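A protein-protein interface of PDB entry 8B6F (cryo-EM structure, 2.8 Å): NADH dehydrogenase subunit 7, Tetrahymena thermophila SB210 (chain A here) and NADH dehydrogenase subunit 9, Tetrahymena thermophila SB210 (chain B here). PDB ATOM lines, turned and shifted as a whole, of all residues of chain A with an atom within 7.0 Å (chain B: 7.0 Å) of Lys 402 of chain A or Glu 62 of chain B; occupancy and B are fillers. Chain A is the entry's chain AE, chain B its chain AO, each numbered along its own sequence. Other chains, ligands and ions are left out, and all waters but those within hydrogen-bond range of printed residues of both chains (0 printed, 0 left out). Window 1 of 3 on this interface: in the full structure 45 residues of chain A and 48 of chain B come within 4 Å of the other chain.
Tyr 376 of chain A touches Ile 61 of chain B.
Tyr 376 of chain A touches Asn 99 of chain B (CE2 to ND2, 3.7 Å).
Ser 389 of chain A touches Phe 97 of chain B.
CD of Lys 402 of chain A touches OG of Ser 64 of chain B, at 3.5 Å.
OE2 of Glu 138 of chain B touches CE of Lys 402 of chain A (3.8 Å).
NE of Arg 404 of chain A touches CG2 of Ile 61 of chain B, at 3.4 Å.
Glu 62 of chain B touches Arg 404 of chain A.
Leu 135 of chain B touches Leu 408 of chain A (CD2 to CD2, 3.99 Å).
His 409 of chain A touches Asn 131 of chain B.
NE2 of His 409 of chain A touches CD1 of Leu 135 of chain B, 3.9 Å away.
Of the 17 printed residues of chain B, 10 touch a printed residue of chain A.
Hydrophobic or aromatic side chains of chain B that line the printed part of chain A: Ile 61, Phe 97, Leu 135 and Tyr 143.
Of the 18 printed residues of chain A, 8 touch a printed residue of chain B.
Hydrophobic or aromatic side chains of chain A that line the printed part of chain B: Tyr 374, Tyr 376, Leu 408 and His 409.
Among the printed residues, Asp or Glu carboxylates within 4 Å of a Lys or Arg side-chain nitrogen of the other chain: Lys 402 of chain A with Glu 62 of chain B (2.6 Å).
Lys 402 of chain A touches just these residues of chain B: Glu 62 (2.6 Å), Ser 64 (3.5 Å) and Glu 138 (3.8 Å).
Of chain A, only Lys 402 and Arg 404 come within 4 Å of Glu 62 of chain B.
Printed residues of chain A within 4 Å of Leu 135 of chain B: Leu 408 (3.99 Å) and His 409 (3.9 Å).
Of the printed residues of chain B, Tyr 374 of chain A touches Phe 97 (3.96 Å).
Printed residues of chain B within 4 Å of His 409 of chain A: Ile 61, Asn 131 and Leu 135.
Tyr 98 of chain B touches none of the printed residues of chain A.
Met 390 of chain A touches none of the printed residues of chain B.
The nearest residue of chain B that does not touch Lys 402 of chain A is Asn 63 of chain B (4.05 Å).
The nearest residue of chain A that does not touch Glu 62 of chain B is Val 403 of chain A (4.2 Å).
The nearest printed residue of chain B that does not touch Ser 389 of chain A is Glu 62 of chain B (5.5 Å).
The side-chain hydroxyl of Ser 64 of chain B lies within hydrogen-bond range of the side-chain amino group of Lys 400 of chain A.
O of Ala 65 of chain B lies within hydrogen-bond range of NZ of Lys 400 of chain A (2.9 Å).
The side-chain hydroxyl of Tyr 143 of chain B lies within hydrogen-bond range of the side-chain amino group of Lys 400 of chain A.
OE2 of Glu 62 of chain B lies within salt-bridge range of NZ of Lys 402 of chain A.
The backbone carbonyl oxygen of Ile 61 of chain B lies within hydrogen-bond range of a ring nitrogen (NE2) of His 409 of chain A (3.1 Å).
The backbone NH (N) of Arg 404 of chain A lies within hydrogen-bond range of the backbone carbonyl oxygen (O) of Gly 387 of chain A (2.9 Å).
O of Lys 400 of chain A lies within hydrogen-bond range of N of Leu 391 of chain A (2.9 Å).
NH1 of Arg 404 of chain A lies within hydrogen-bond range of ND1 of His 409 of chain A, at 3.1 Å.
The backbone carbonyl oxygen of Leu 60 of chain B is in hydrogen-bond range of the side-chain amide nitrogen of Asn 131 of chain B.
The backbone NH of Ile 61 of chain B is in hydrogen-bond range of the backbone carbonyl oxygen of Asn 99 of chain B (2.8 Å).
The backbone carbonyl oxygen (O) of Ser 64 of chain B lies within hydrogen-bond range of the backbone NH (N) of Phe 97 of chain B (2.9 Å).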
ATOM      1  N   GLU A  67      -7.956 -35.156 -29.322  1.00  0.00           N
ATOM      2  CA  GLU A  67      -7.553 -34.337 -30.459  1.00  0.00           C
ATOM      3  C   GLU A  67      -6.684 -35.131 -31.425  1.00  0.00           C
ATOM      4  O   GLU A  67      -6.814 -34.988 -32.646  1.00  0.00           O
ATOM      5  CB  GLU A  67      -6.825 -33.089 -29.968  1.00  0.00           C
ATOM      6  CG  GLU A  67      -7.662 -32.237 -29.027  1.00  0.00           C
ATOM      7  CD  GLU A  67      -6.909 -31.033 -28.506  1.00  0.00           C
ATOM      8  OE1 GLU A  67      -5.754 -30.824 -28.934  1.00  0.00           O
ATOM      9  OE2 GLU A  67      -7.470 -30.298 -27.666  1.00  0.00           O
ATOM     10  N   GLU A  71      -7.649 -35.899 -35.328  1.00  0.00           N
ATOM     11  CA  GLU A  71      -6.751 -35.649 -36.449  1.00  0.00           C
ATOM     12  C   GLU A  71      -6.553 -36.907 -37.283  1.00  0.00           C
ATOM     13  O   GLU A  71      -6.489 -36.842 -38.516  1.00  0.00           O
ATOM     14  CB  GLU A  71      -5.405 -35.132 -35.940  1.00  0.00           C
ATOM     15  CG  GLU A  71      -5.458 -33.734 -35.348  1.00  0.00           C
ATOM     16  CD  GLU A  71      -4.100 -33.259 -34.869  1.00  0.00           C
ATOM     17  OE1 GLU A  71      -3.095 -33.934 -35.170  1.00  0.00           O
ATOM     18  OE2 GLU A  71      -4.038 -32.215 -34.186  1.00  0.00           O
ATOM     19  N   PHE A  82     -16.796 -35.199 -29.427  1.00  0.00           N
ATOM     20  CA  PHE A  82     -17.377 -34.000 -28.836  1.00  0.00           C
ATOM     21  C   PHE A  82     -18.520 -34.335 -27.891  1.00  0.00           C
ATOM     22  O   PHE A  82     -18.722 -33.635 -26.895  1.00  0.00           O
ATOM     23  CB  PHE A  82     -17.823 -33.047 -29.938  1.00  0.00           C
ATOM     24  CG  PHE A  82     -16.681 -32.370 -30.626  1.00  0.00           C
ATOM     25  CD1 PHE A  82     -15.956 -33.028 -31.601  1.00  0.00           C
ATOM     26  CD2 PHE A  82     -16.315 -31.083 -30.276  1.00  0.00           C
ATOM     27  CE1 PHE A  82     -14.892 -32.410 -32.225  1.00  0.00           C
ATOM     28  CE2 PHE A  82     -15.255 -30.460 -30.894  1.00  0.00           C
ATOM     29  CZ  PHE A  82     -14.540 -31.122 -31.871  1.00  0.00           C
ATOM     30  N   TYR A 374      -8.471 -21.857 -41.820  1.00  0.00           N
ATOM     31  CA  TYR A 374      -8.503 -21.807 -40.365  1.00  0.00           C
ATOM     32  C   TYR A 374      -9.799 -21.150 -39.914  1.00  0.00           C
ATOM     33  O   TYR A 374     -10.198 -20.119 -40.463  1.00  0.00           O
ATOM     34  CB  TYR A 374      -7.303 -21.034 -39.817  1.00  0.00           C
ATOM     35  CG  TYR A 374      -7.422 -20.685 -38.351  1.00  0.00           C
ATOM     36  CD1 TYR A 374      -7.123 -21.618 -37.368  1.00  0.00           C
ATOM     37  CD2 TYR A 374      -7.830 -19.420 -37.952  1.00  0.00           C
ATOM     38  CE1 TYR A 374      -7.232 -21.302 -36.029  1.00  0.00           C
ATOM     39  CE2 TYR A 374      -7.941 -19.093 -36.616  1.00  0.00           C
ATOM     40  CZ  TYR A 374      -7.641 -20.038 -35.659  1.00  0.00           C
ATOM     41  OH  TYR A 374      -7.751 -19.714 -34.327  1.00  0.00           O
ATOM     42  N   TYR A 376     -12.413 -20.494 -36.174  1.00  0.00           N
ATOM     43  CA  TYR A 376     -12.663 -20.620 -34.742  1.00  0.00           C
ATOM     44  C   TYR A 376     -14.134 -20.308 -34.511  1.00  0.00           C
ATOM     45  O   TYR A 376     -14.557 -19.160 -34.673  1.00  0.00           O
ATOM     46  CB  TYR A 376     -11.771 -19.688 -33.922  1.00  0.00           C
ATOM     47  CG  TYR A 376     -12.188 -19.601 -32.472  1.00  0.00           C
ATOM     48  CD1 TYR A 376     -11.830 -20.590 -31.566  1.00  0.00           C
ATOM     49  CD2 TYR A 376     -12.949 -18.538 -32.013  1.00  0.00           C
ATOM     50  CE1 TYR A 376     -12.213 -20.519 -30.244  1.00  0.00           C
ATOM     51  CE2 TYR A 376     -13.338 -18.457 -30.692  1.00  0.00           C
ATOM     52  CZ  TYR A 376     -12.967 -19.451 -29.813  1.00  0.00           C
ATOM     53  OH  TYR A 376     -13.352 -19.374 -28.495  1.00  0.00           O
ATOM     54  N   GLY A 387     -15.524 -23.630 -27.548  1.00  0.00           N
ATOM     55  CA  GLY A 387     -15.115 -23.288 -28.889  1.00  0.00           C
ATOM     56  C   GLY A 387     -14.270 -24.379 -29.517  1.00  0.00           C
ATOM     57  O   GLY A 387     -13.669 -25.208 -28.837  1.00  0.00           O
ATOM     58  N   VAL A 388     -14.242 -24.360 -30.846  1.00  0.00           N
ATOM     59  CA  VAL A 388     -13.410 -25.254 -31.639  1.00  0.00           C
ATOM     60  C   VAL A 388     -12.586 -24.406 -32.594  1.00  0.00           C
ATOM     61  O   VAL A 388     -13.132 -23.561 -33.311  1.00  0.00           O
ATOM     62  CB  VAL A 388     -14.247 -26.295 -32.410  1.00  0.00           C
ATOM     63  CG1 VAL A 388     -15.056 -27.139 -31.446  1.00  0.00           C
ATOM     64  CG2 VAL A 388     -15.168 -25.624 -33.421  1.00  0.00           C
ATOM     65  N   SER A 389     -11.276 -24.614 -32.582  1.00  0.00           N
ATOM     66  CA  SER A 389     -10.352 -23.952 -33.495  1.00  0.00           C
ATOM     67  C   SER A 389      -9.795 -25.020 -34.424  1.00  0.00           C
ATOM     68  O   SER A 389      -8.951 -25.824 -34.018  1.00  0.00           O
ATOM     69  CB  SER A 389      -9.242 -23.244 -32.721  1.00  0.00           C
ATOM     70  OG  SER A 389      -8.397 -22.512 -33.590  1.00  0.00           O
ATOM     71  N   MET A 390     -10.261 -25.022 -35.670  1.00  0.00           N
ATOM     72  CA  MET A 390      -9.948 -26.071 -36.631  1.00  0.00           C
ATOM     73  C   MET A 390      -9.140 -25.502 -37.786  1.00  0.00           C
ATOM     74  O   MET A 390      -9.507 -24.473 -38.361  1.00  0.00           O
ATOM     75  CB  MET A 390     -11.222 -26.730 -37.163  1.00  0.00           C
ATOM     76  CG  MET A 390     -11.918 -27.612 -36.144  1.00  0.00           C
ATOM     77  SD  MET A 390     -13.160 -28.693 -36.878  1.00  0.00           S
ATOM     78  CE  MET A 390     -14.302 -27.491 -37.544  1.00  0.00           C
ATOM     79  N   LEU A 391      -8.044 -26.176 -38.113  1.00  0.00           N
ATOM     80  CA  LEU A 391      -7.234 -25.874 -39.284  1.00  0.00           C
ATOM     81  C   LEU A 391      -7.324 -27.055 -40.239  1.00  0.00           C
ATOM     82  O   LEU A 391      -6.959 -28.179 -39.878  1.00  0.00           O
ATOM     83  CB  LEU A 391      -5.782 -25.602 -38.895  1.00  0.00           C
ATOM     84  CG  LEU A 391      -4.805 -25.395 -40.054  1.00  0.00           C
ATOM     85  CD1 LEU A 391      -5.187 -24.190 -40.889  1.00  0.00           C
ATOM     86  CD2 LEU A 391      -3.395 -25.247 -39.525  1.00  0.00           C
ATOM     87  N   LYS A 400      -5.629 -29.887 -37.800  1.00  0.00           N
ATOM     88  CA  LYS A 400      -5.600 -29.635 -36.369  1.00  0.00           C
ATOM     89  C   LYS A 400      -7.003 -29.282 -35.902  1.00  0.00           C
ATOM     90  O   LYS A 400      -7.786 -28.683 -36.642  1.00  0.00           O
ATOM     91  CB  LYS A 400      -4.629 -28.507 -36.013  1.00  0.00           C
ATOM     92  CG  LYS A 400      -4.639 -28.154 -34.538  1.00  0.00           C
ATOM     93  CD  LYS A 400      -3.689 -27.023 -34.224  1.00  0.00           C
ATOM     94  CE  LYS A 400      -3.862 -26.574 -32.790  1.00  0.00           C
ATOM     95  NZ  LYS A 400      -3.578 -27.704 -31.865  1.00  0.00           N
ATOM     96  N   CYS A 401      -7.312 -29.666 -34.663  1.00  0.00           N
ATOM     97  CA  CYS A 401      -8.607 -29.351 -34.064  1.00  0.00           C
ATOM     98  C   CYS A 401      -8.383 -29.150 -32.568  1.00  0.00           C
ATOM     99  O   CYS A 401      -8.360 -30.122 -31.809  1.00  0.00           O
ATOM    100  CB  CYS A 401      -9.620 -30.454 -34.338  1.00  0.00           C
ATOM    101  SG  CYS A 401     -11.240 -30.181 -33.591  1.00  0.00           S
ATOM    102  N   LYS A 402      -8.217 -27.895 -32.158  1.00  0.00           N
ATOM    103  CA  LYS A 402      -8.084 -27.550 -30.750  1.00  0.00           C
ATOM    104  C   LYS A 402      -9.458 -27.250 -30.166  1.00  0.00           C
ATOM    105  O   LYS A 402     -10.317 -26.676 -30.838  1.00  0.00           O
ATOM    106  CB  LYS A 402      -7.159 -26.344 -30.574  1.00  0.00           C
ATOM    107  CG  LYS A 402      -6.882 -25.960 -29.125  1.00  0.00           C
ATOM    108  CD  LYS A 402      -6.101 -27.046 -28.398  1.00  0.00           C
ATOM    109  CE  LYS A 402      -5.771 -26.642 -26.970  1.00  0.00           C
ATOM    110  NZ  LYS A 402      -6.990 -26.390 -26.153  1.00  0.00           N
ATOM    111  N   VAL A 403      -9.659 -27.641 -28.912  1.00  0.00           N
ATOM    112  CA  VAL A 403     -10.938 -27.484 -28.229  1.00  0.00           C
ATOM    113  C   VAL A 403     -10.736 -26.554 -27.042  1.00  0.00           C
ATOM    114  O   VAL A 403      -9.991 -26.881 -26.111  1.00  0.00           O
ATOM    115  CB  VAL A 403     -11.511 -28.835 -27.776  1.00  0.00           C
ATOM    116  CG1 VAL A 403     -12.841 -28.641 -27.064  1.00  0.00           C
ATOM    117  CG2 VAL A 403     -11.675 -29.762 -28.966  1.00  0.00           C
ATOM    118  N   ARG A 404     -11.403 -25.404 -27.073  1.00  0.00           N
ATOM    119  CA  ARG A 404     -11.403 -24.471 -25.953  1.00  0.00           C
ATOM    120  C   ARG A 404     -12.580 -24.821 -25.051  1.00  0.00           C
ATOM    121  O   ARG A 404     -13.735 -24.544 -25.389  1.00  0.00           O
ATOM    122  CB  ARG A 404     -11.491 -23.032 -26.455  1.00  0.00           C
ATOM    123  CG  ARG A 404     -11.517 -21.973 -25.360  1.00  0.00           C
ATOM    124  CD  ARG A 404     -12.932 -21.647 -24.918  1.00  0.00           C
ATOM    125  NE  ARG A 404     -12.977 -20.478 -24.049  1.00  0.00           N
ATOM    126  CZ  ARG A 404     -12.793 -20.507 -22.736  1.00  0.00           C
ATOM    127  NH1 ARG A 404     -12.537 -21.637 -22.098  1.00  0.00           N
ATOM    128  NH2 ARG A 404     -12.867 -19.374 -22.046  1.00  0.00           N
ATOM    129  N   SER A 405     -12.287 -25.431 -23.909  1.00  0.00           N
ATOM    130  CA  SER A 405     -13.311 -25.868 -22.971  1.00  0.00           C
ATOM    131  C   SER A 405     -13.384 -24.915 -21.791  1.00  0.00           C
ATOM    132  O   SER A 405     -12.348 -24.636 -21.172  1.00  0.00           O
ATOM    133  CB  SER A 405     -13.015 -27.279 -22.475  1.00  0.00           C
ATOM    134  OG  SER A 405     -11.760 -27.334 -21.823  1.00  0.00           O
ATOM    135  N   LEU A 408     -11.779 -26.123 -18.148  1.00  0.00           N
ATOM    136  CA  LEU A 408     -10.380 -25.949 -17.774  1.00  0.00           C
ATOM    137  C   LEU A 408     -10.154 -24.589 -17.126  1.00  0.00           C
ATOM    138  O   LEU A 408      -9.506 -24.488 -16.077  1.00  0.00           O
ATOM    139  CB  LEU A 408      -9.491 -26.112 -19.006  1.00  0.00           C
ATOM    140  CG  LEU A 408      -7.981 -26.045 -18.768  1.00  0.00           C
ATOM    141  CD1 LEU A 408      -7.502 -27.264 -18.000  1.00  0.00           C
ATOM    142  CD2 LEU A 408      -7.237 -25.916 -20.083  1.00  0.00           C
ATOM    143  N   HIS A 409     -10.683 -23.527 -17.735  1.00  0.00           N
ATOM    144  CA  HIS A 409     -10.507 -22.192 -17.173  1.00  0.00           C
ATOM    145  C   HIS A 409     -11.229 -22.053 -15.839  1.00  0.00           C
ATOM    146  O   HIS A 409     -10.734 -21.382 -14.927  1.00  0.00           O
ATOM    147  CB  HIS A 409     -10.993 -21.137 -18.165  1.00  0.00           C
ATOM    148  CG  HIS A 409     -10.177 -21.068 -19.418  1.00  0.00           C
ATOM    149  ND1 HIS A 409     -10.102 -22.109 -20.319  1.00  0.00           N
ATOM    150  CD2 HIS A 409      -9.397 -20.082 -19.919  1.00  0.00           C
ATOM    151  CE1 HIS A 409      -9.313 -21.765 -21.319  1.00  0.00           C
ATOM    152  NE2 HIS A 409      -8.872 -20.540 -21.102  1.00  0.00           N
ATOM    153  N   THR B  59      -9.267 -10.688 -22.328  1.00  0.00           N
ATOM    154  CA  THR B  59      -9.089 -11.991 -21.703  1.00  0.00           C
ATOM    155  C   THR B  59      -8.523 -12.967 -22.723  1.00  0.00           C
ATOM    156  O   THR B  59      -8.969 -13.004 -23.872  1.00  0.00           O
ATOM    157  CB  THR B  59     -10.404 -12.555 -21.154  1.00  0.00           C
ATOM    158  OG1 THR B  59     -11.234 -12.993 -22.237  1.00  0.00           O
ATOM    159  CG2 THR B  59     -11.142 -11.511 -20.365  1.00  0.00           C
ATOM    160  N   LEU B  60      -7.540 -13.754 -22.298  1.00  0.00           N
ATOM    161  CA  LEU B  60      -6.909 -14.747 -23.163  1.00  0.00           C
ATOM    162  C   LEU B  60      -7.832 -15.956 -23.224  1.00  0.00           C
ATOM    163  O   LEU B  60      -7.843 -16.793 -22.319  1.00  0.00           O
ATOM    164  CB  LEU B  60      -5.523 -15.111 -22.643  1.00  0.00           C
ATOM    165  CG  LEU B  60      -4.590 -15.826 -23.620  1.00  0.00           C
ATOM    166  CD1 LEU B  60      -3.157 -15.707 -23.151  1.00  0.00           C
ATOM    167  CD2 LEU B  60      -4.960 -17.288 -23.782  1.00  0.00           C
ATOM    168  N   ILE B  61      -8.625 -16.040 -24.291  1.00  0.00           N
ATOM    169  CA  ILE B  61      -9.592 -17.126 -24.421  1.00  0.00           C
ATOM    170  C   ILE B  61      -8.888 -18.460 -24.645  1.00  0.00           C
ATOM    171  O   ILE B  61      -9.223 -19.466 -24.010  1.00  0.00           O
ATOM    172  CB  ILE B  61     -10.588 -16.812 -25.553  1.00  0.00           C
ATOM    173  CG1 ILE B  61     -11.405 -15.557 -25.223  1.00  0.00           C
ATOM    174  CG2 ILE B  61     -11.506 -17.999 -25.818  1.00  0.00           C
ATOM    175  CD1 ILE B  61     -12.330 -15.697 -24.026  1.00  0.00           C
ATOM    176  N   GLU B  62      -7.910 -18.497 -25.546  1.00  0.00           N
ATOM    177  CA  GLU B  62      -7.344 -19.770 -25.967  1.00  0.00           C
ATOM    178  C   GLU B  62      -5.884 -19.593 -26.358  1.00  0.00           C
ATOM    179  O   GLU B  62      -5.424 -18.487 -26.648  1.00  0.00           O
ATOM    180  CB  GLU B  62      -8.152 -20.357 -27.135  1.00  0.00           C
ATOM    181  CG  GLU B  62      -7.682 -21.716 -27.644  1.00  0.00           C
ATOM    182  CD  GLU B  62      -7.703 -22.793 -26.573  1.00  0.00           C
ATOM    183  OE1 GLU B  62      -8.255 -22.546 -25.483  1.00  0.00           O
ATOM    184  OE2 GLU B  62      -7.171 -23.894 -26.827  1.00  0.00           O
ATOM    185  N   ASN B  63      -5.164 -20.713 -26.364  1.00  0.00           N
ATOM    186  CA  ASN B  63      -3.767 -20.760 -26.770  1.00  0.00           C
ATOM    187  C   ASN B  63      -3.432 -22.194 -27.145  1.00  0.00           C
ATOM    188  O   ASN B  63      -3.832 -23.127 -26.447  1.00  0.00           O
ATOM    189  CB  ASN B  63      -2.846 -20.270 -25.649  1.00  0.00           C
ATOM    190  CG  ASN B  63      -1.410 -20.708 -25.842  1.00  0.00           C
ATOM    191  OD1 ASN B  63      -0.938 -20.859 -26.967  1.00  0.00           O
ATOM    192  ND2 ASN B  63      -0.707 -20.920 -24.738  1.00  0.00           N
ATOM    193  N   SER B  64      -2.701 -22.364 -28.237  1.00  0.00           N
ATOM    194  CA  SER B  64      -2.297 -23.693 -28.687  1.00  0.00           C
ATOM    195  C   SER B  64      -1.191 -23.530 -29.725  1.00  0.00           C
ATOM    196  O   SER B  64      -0.669 -22.429 -29.932  1.00  0.00           O
ATOM    197  CB  SER B  64      -3.497 -24.469 -29.224  1.00  0.00           C
ATOM    198  OG  SER B  64      -3.118 -25.755 -29.666  1.00  0.00           O
ATOM    199  N   ALA B  65      -0.833 -24.635 -30.381  1.00  0.00           N
ATOM    200  CA  ALA B  65       0.246 -24.650 -31.358  1.00  0.00           C
ATOM    201  C   ALA B  65      -0.095 -25.610 -32.489  1.00  0.00           C
ATOM    202  O   ALA B  65      -0.927 -26.506 -32.342  1.00  0.00           O
ATOM    203  CB  ALA B  65       1.579 -25.054 -30.717  1.00  0.00           C
ATOM    204  N   PHE B  97      -0.266 -20.127 -31.591  1.00  0.00           N
ATOM    205  CA  PHE B  97      -1.285 -19.102 -31.767  1.00  0.00           C
ATOM    206  C   PHE B  97      -2.029 -18.865 -30.461  1.00  0.00           C
ATOM    207  O   PHE B  97      -2.372 -19.812 -29.749  1.00  0.00           O
ATOM    208  CB  PHE B  97      -2.264 -19.473 -32.891  1.00  0.00           C
ATOM    209  CG  PHE B  97      -3.237 -20.551 -32.527  1.00  0.00           C
ATOM    210  CD1 PHE B  97      -4.438 -20.243 -31.908  1.00  0.00           C
ATOM    211  CD2 PHE B  97      -2.974 -21.871 -32.846  1.00  0.00           C
ATOM    212  CE1 PHE B  97      -5.340 -21.236 -31.585  1.00  0.00           C
ATOM    213  CE2 PHE B  97      -3.871 -22.867 -32.527  1.00  0.00           C
ATOM    214  CZ  PHE B  97      -5.057 -22.549 -31.898  1.00  0.00           C
ATOM    215  N   TYR B  98      -2.265 -17.593 -30.157  1.00  0.00           N
ATOM    216  CA  TYR B  98      -3.046 -17.166 -29.006  1.00  0.00           C
ATOM    217  C   TYR B  98      -4.287 -16.433 -29.492  1.00  0.00           C
ATOM    218  O   TYR B  98      -4.282 -15.819 -30.561  1.00  0.00           O
ATOM    219  CB  TYR B  98      -2.238 -16.257 -28.073  1.00  0.00           C
ATOM    220  CG  TYR B  98      -1.006 -16.911 -27.496  1.00  0.00           C
ATOM    221  CD1 TYR B  98       0.106 -17.169 -28.288  1.00  0.00           C
ATOM    222  CD2 TYR B  98      -0.948 -17.259 -26.154  1.00  0.00           C
ATOM    223  CE1 TYR B  98       1.234 -17.762 -27.762  1.00  0.00           C
ATOM    224  CE2 TYR B  98       0.176 -17.854 -25.618  1.00  0.00           C
ATOM    225  CZ  TYR B  98       1.264 -18.102 -26.428  1.00  0.00           C
ATOM    226  OH  TYR B  98       2.386 -18.692 -25.900  1.00  0.00           O
ATOM    227  N   ASN B  99      -5.352 -16.497 -28.699  1.00  0.00           N
ATOM    228  CA  ASN B  99      -6.616 -15.867 -29.053  1.00  0.00           C
ATOM    229  C   ASN B  99      -7.184 -15.169 -27.830  1.00  0.00           C
ATOM    230  O   ASN B  99      -7.371 -15.794 -26.783  1.00  0.00           O
ATOM    231  CB  ASN B  99      -7.610 -16.903 -29.589  1.00  0.00           C
ATOM    232  CG  ASN B  99      -8.978 -16.313 -29.857  1.00  0.00           C
ATOM    233  OD1 ASN B  99      -9.110 -15.119 -30.121  1.00  0.00           O
ATOM    234  ND2 ASN B  99     -10.005 -17.151 -29.795  1.00  0.00           N
ATOM    235  N   TYR B 100      -7.472 -13.878 -27.977  1.00  0.00           N
ATOM    236  CA  TYR B 100      -8.005 -13.051 -26.907  1.00  0.00           C
ATOM    237  C   TYR B 100      -9.341 -12.453 -27.327  1.00  0.00           C
ATOM    238  O   TYR B 100      -9.658 -12.348 -28.514  1.00  0.00           O
ATOM    239  CB  TYR B 100      -7.046 -11.910 -26.537  1.00  0.00           C
ATOM    240  CG  TYR B 100      -5.577 -12.269 -26.547  1.00  0.00           C
ATOM    241  CD1 TYR B 100      -4.871 -12.356 -27.738  1.00  0.00           C
ATOM    242  CD2 TYR B 100      -4.888 -12.478 -25.361  1.00  0.00           C
ATOM    243  CE1 TYR B 100      -3.528 -12.667 -27.750  1.00  0.00           C
ATOM    244  CE2 TYR B 100      -3.546 -12.790 -25.363  1.00  0.00           C
ATOM    245  CZ  TYR B 100      -2.872 -12.882 -26.560  1.00  0.00           C
ATOM    246  OH  TYR B 100      -1.532 -13.190 -26.567  1.00  0.00           O
ATOM    247  N   TYR B 101     -10.123 -12.059 -26.326  1.00  0.00           N
ATOM    248  CA  TYR B 101     -11.381 -11.352 -26.526  1.00  0.00           C
ATOM    249  C   TYR B 101     -11.347 -10.051 -25.737  1.00  0.00           C
ATOM    250  O   TYR B 101     -11.010 -10.049 -24.549  1.00  0.00           O
ATOM    251  CB  TYR B 101     -12.575 -12.202 -26.094  1.00  0.00           C
ATOM    252  CG  TYR B 101     -13.892 -11.477 -26.224  1.00  0.00           C
ATOM    253  CD1 TYR B 101     -14.524 -11.369 -27.454  1.00  0.00           C
ATOM    254  CD2 TYR B 101     -14.500 -10.899 -25.120  1.00  0.00           C
ATOM    255  CE1 TYR B 101     -15.724 -10.706 -27.582  1.00  0.00           C
ATOM    256  CE2 TYR B 101     -15.701 -10.233 -25.239  1.00  0.00           C
ATOM    257  CZ  TYR B 101     -16.308 -10.140 -26.473  1.00  0.00           C
ATOM    258  OH  TYR B 101     -17.506  -9.477 -26.595  1.00  0.00           O
ATOM    259  N   ASN B 131      -4.672 -17.234 -16.589  1.00  0.00           N
ATOM    260  CA  ASN B 131      -5.172 -18.492 -17.131  1.00  0.00           C
ATOM    261  C   ASN B 131      -4.239 -19.097 -18.168  1.00  0.00           C
ATOM    262  O   ASN B 131      -4.439 -20.255 -18.551  1.00  0.00           O
ATOM    263  CB  ASN B 131      -6.558 -18.301 -17.749  1.00  0.00           C
ATOM    264  CG  ASN B 131      -6.552 -17.336 -18.914  1.00  0.00           C
ATOM    265  OD1 ASN B 131      -5.507 -16.820 -19.303  1.00  0.00           O
ATOM    266  ND2 ASN B 131      -7.724 -17.092 -19.481  1.00  0.00           N
ATOM    267  N   LEU B 135      -2.707 -23.445 -19.978  1.00  0.00           N
ATOM    268  CA  LEU B 135      -2.694 -23.486 -21.437  1.00  0.00           C
ATOM    269  C   LEU B 135      -1.279 -23.698 -21.957  1.00  0.00           C
ATOM    270  O   LEU B 135      -1.046 -24.533 -22.836  1.00  0.00           O
ATOM    271  CB  LEU B 135      -3.286 -22.197 -22.007  1.00  0.00           C
ATOM    272  CG  LEU B 135      -4.753 -21.902 -21.689  1.00  0.00           C
ATOM    273  CD1 LEU B 135      -5.139 -20.533 -22.219  1.00  0.00           C
ATOM    274  CD2 LEU B 135      -5.660 -22.974 -22.268  1.00  0.00           C
ATOM    275  N   GLU B 138       0.036 -27.236 -21.100  1.00  0.00           N
ATOM    276  CA  GLU B 138      -0.473 -28.217 -22.053  1.00  0.00           C
ATOM    277  C   GLU B 138       0.242 -28.097 -23.395  1.00  0.00           C
ATOM    278  O   GLU B 138       0.660 -29.101 -23.982  1.00  0.00           O
ATOM    279  CB  GLU B 138      -1.980 -28.034 -22.227  1.00  0.00           C
ATOM    280  CG  GLU B 138      -2.602 -28.944 -23.273  1.00  0.00           C
ATOM    281  CD  GLU B 138      -4.089 -28.704 -23.436  1.00  0.00           C
ATOM    282  OE1 GLU B 138      -4.665 -27.958 -22.616  1.00  0.00           O
ATOM    283  OE2 GLU B 138      -4.682 -29.256 -24.386  1.00  0.00           O
ATOM    284  N   THR B 139       0.396 -26.871 -23.895  1.00  0.00           N
ATOM    285  CA  THR B 139       1.051 -26.675 -25.185  1.00  0.00           C
ATOM    286  C   THR B 139       2.484 -27.186 -25.151  1.00  0.00           C
ATOM    287  O   THR B 139       2.933 -27.879 -26.071  1.00  0.00           O
ATOM    288  CB  THR B 139       1.020 -25.196 -25.572  1.00  0.00           C
ATOM    289  OG1 THR B 139      -0.338 -24.750 -25.655  1.00  0.00           O
ATOM    290  CG2 THR B 139       1.700 -24.973 -26.917  1.00  0.00           C
ATOM    291  N   TYR B 143       3.364 -30.412 -27.519  1.00  0.00           N
ATOM    292  CA  TYR B 143       4.125 -30.063 -28.706  1.00  0.00           C
ATOM    293  C   TYR B 143       5.601 -29.808 -28.437  1.00  0.00           C
ATOM    294  O   TYR B 143       6.362 -29.640 -29.395  1.00  0.00           O
ATOM    295  CB  TYR B 143       3.522 -28.820 -29.380  1.00  0.00           C
ATOM    296  CG  TYR B 143       2.186 -29.075 -30.034  1.00  0.00           C
ATOM    297  CD1 TYR B 143       2.106 -29.522 -31.347  1.00  0.00           C
ATOM    298  CD2 TYR B 143       1.003 -28.866 -29.340  1.00  0.00           C
ATOM    299  CE1 TYR B 143       0.886 -29.756 -31.948  1.00  0.00           C
ATOM    300  CE2 TYR B 143      -0.221 -29.095 -29.931  1.00  0.00           C
ATOM    301  CZ  TYR B 143      -0.274 -29.541 -31.234  1.00  0.00           C
ATOM    302  OH  TYR B 143      -1.493 -29.772 -31.823  1.00  0.00           O
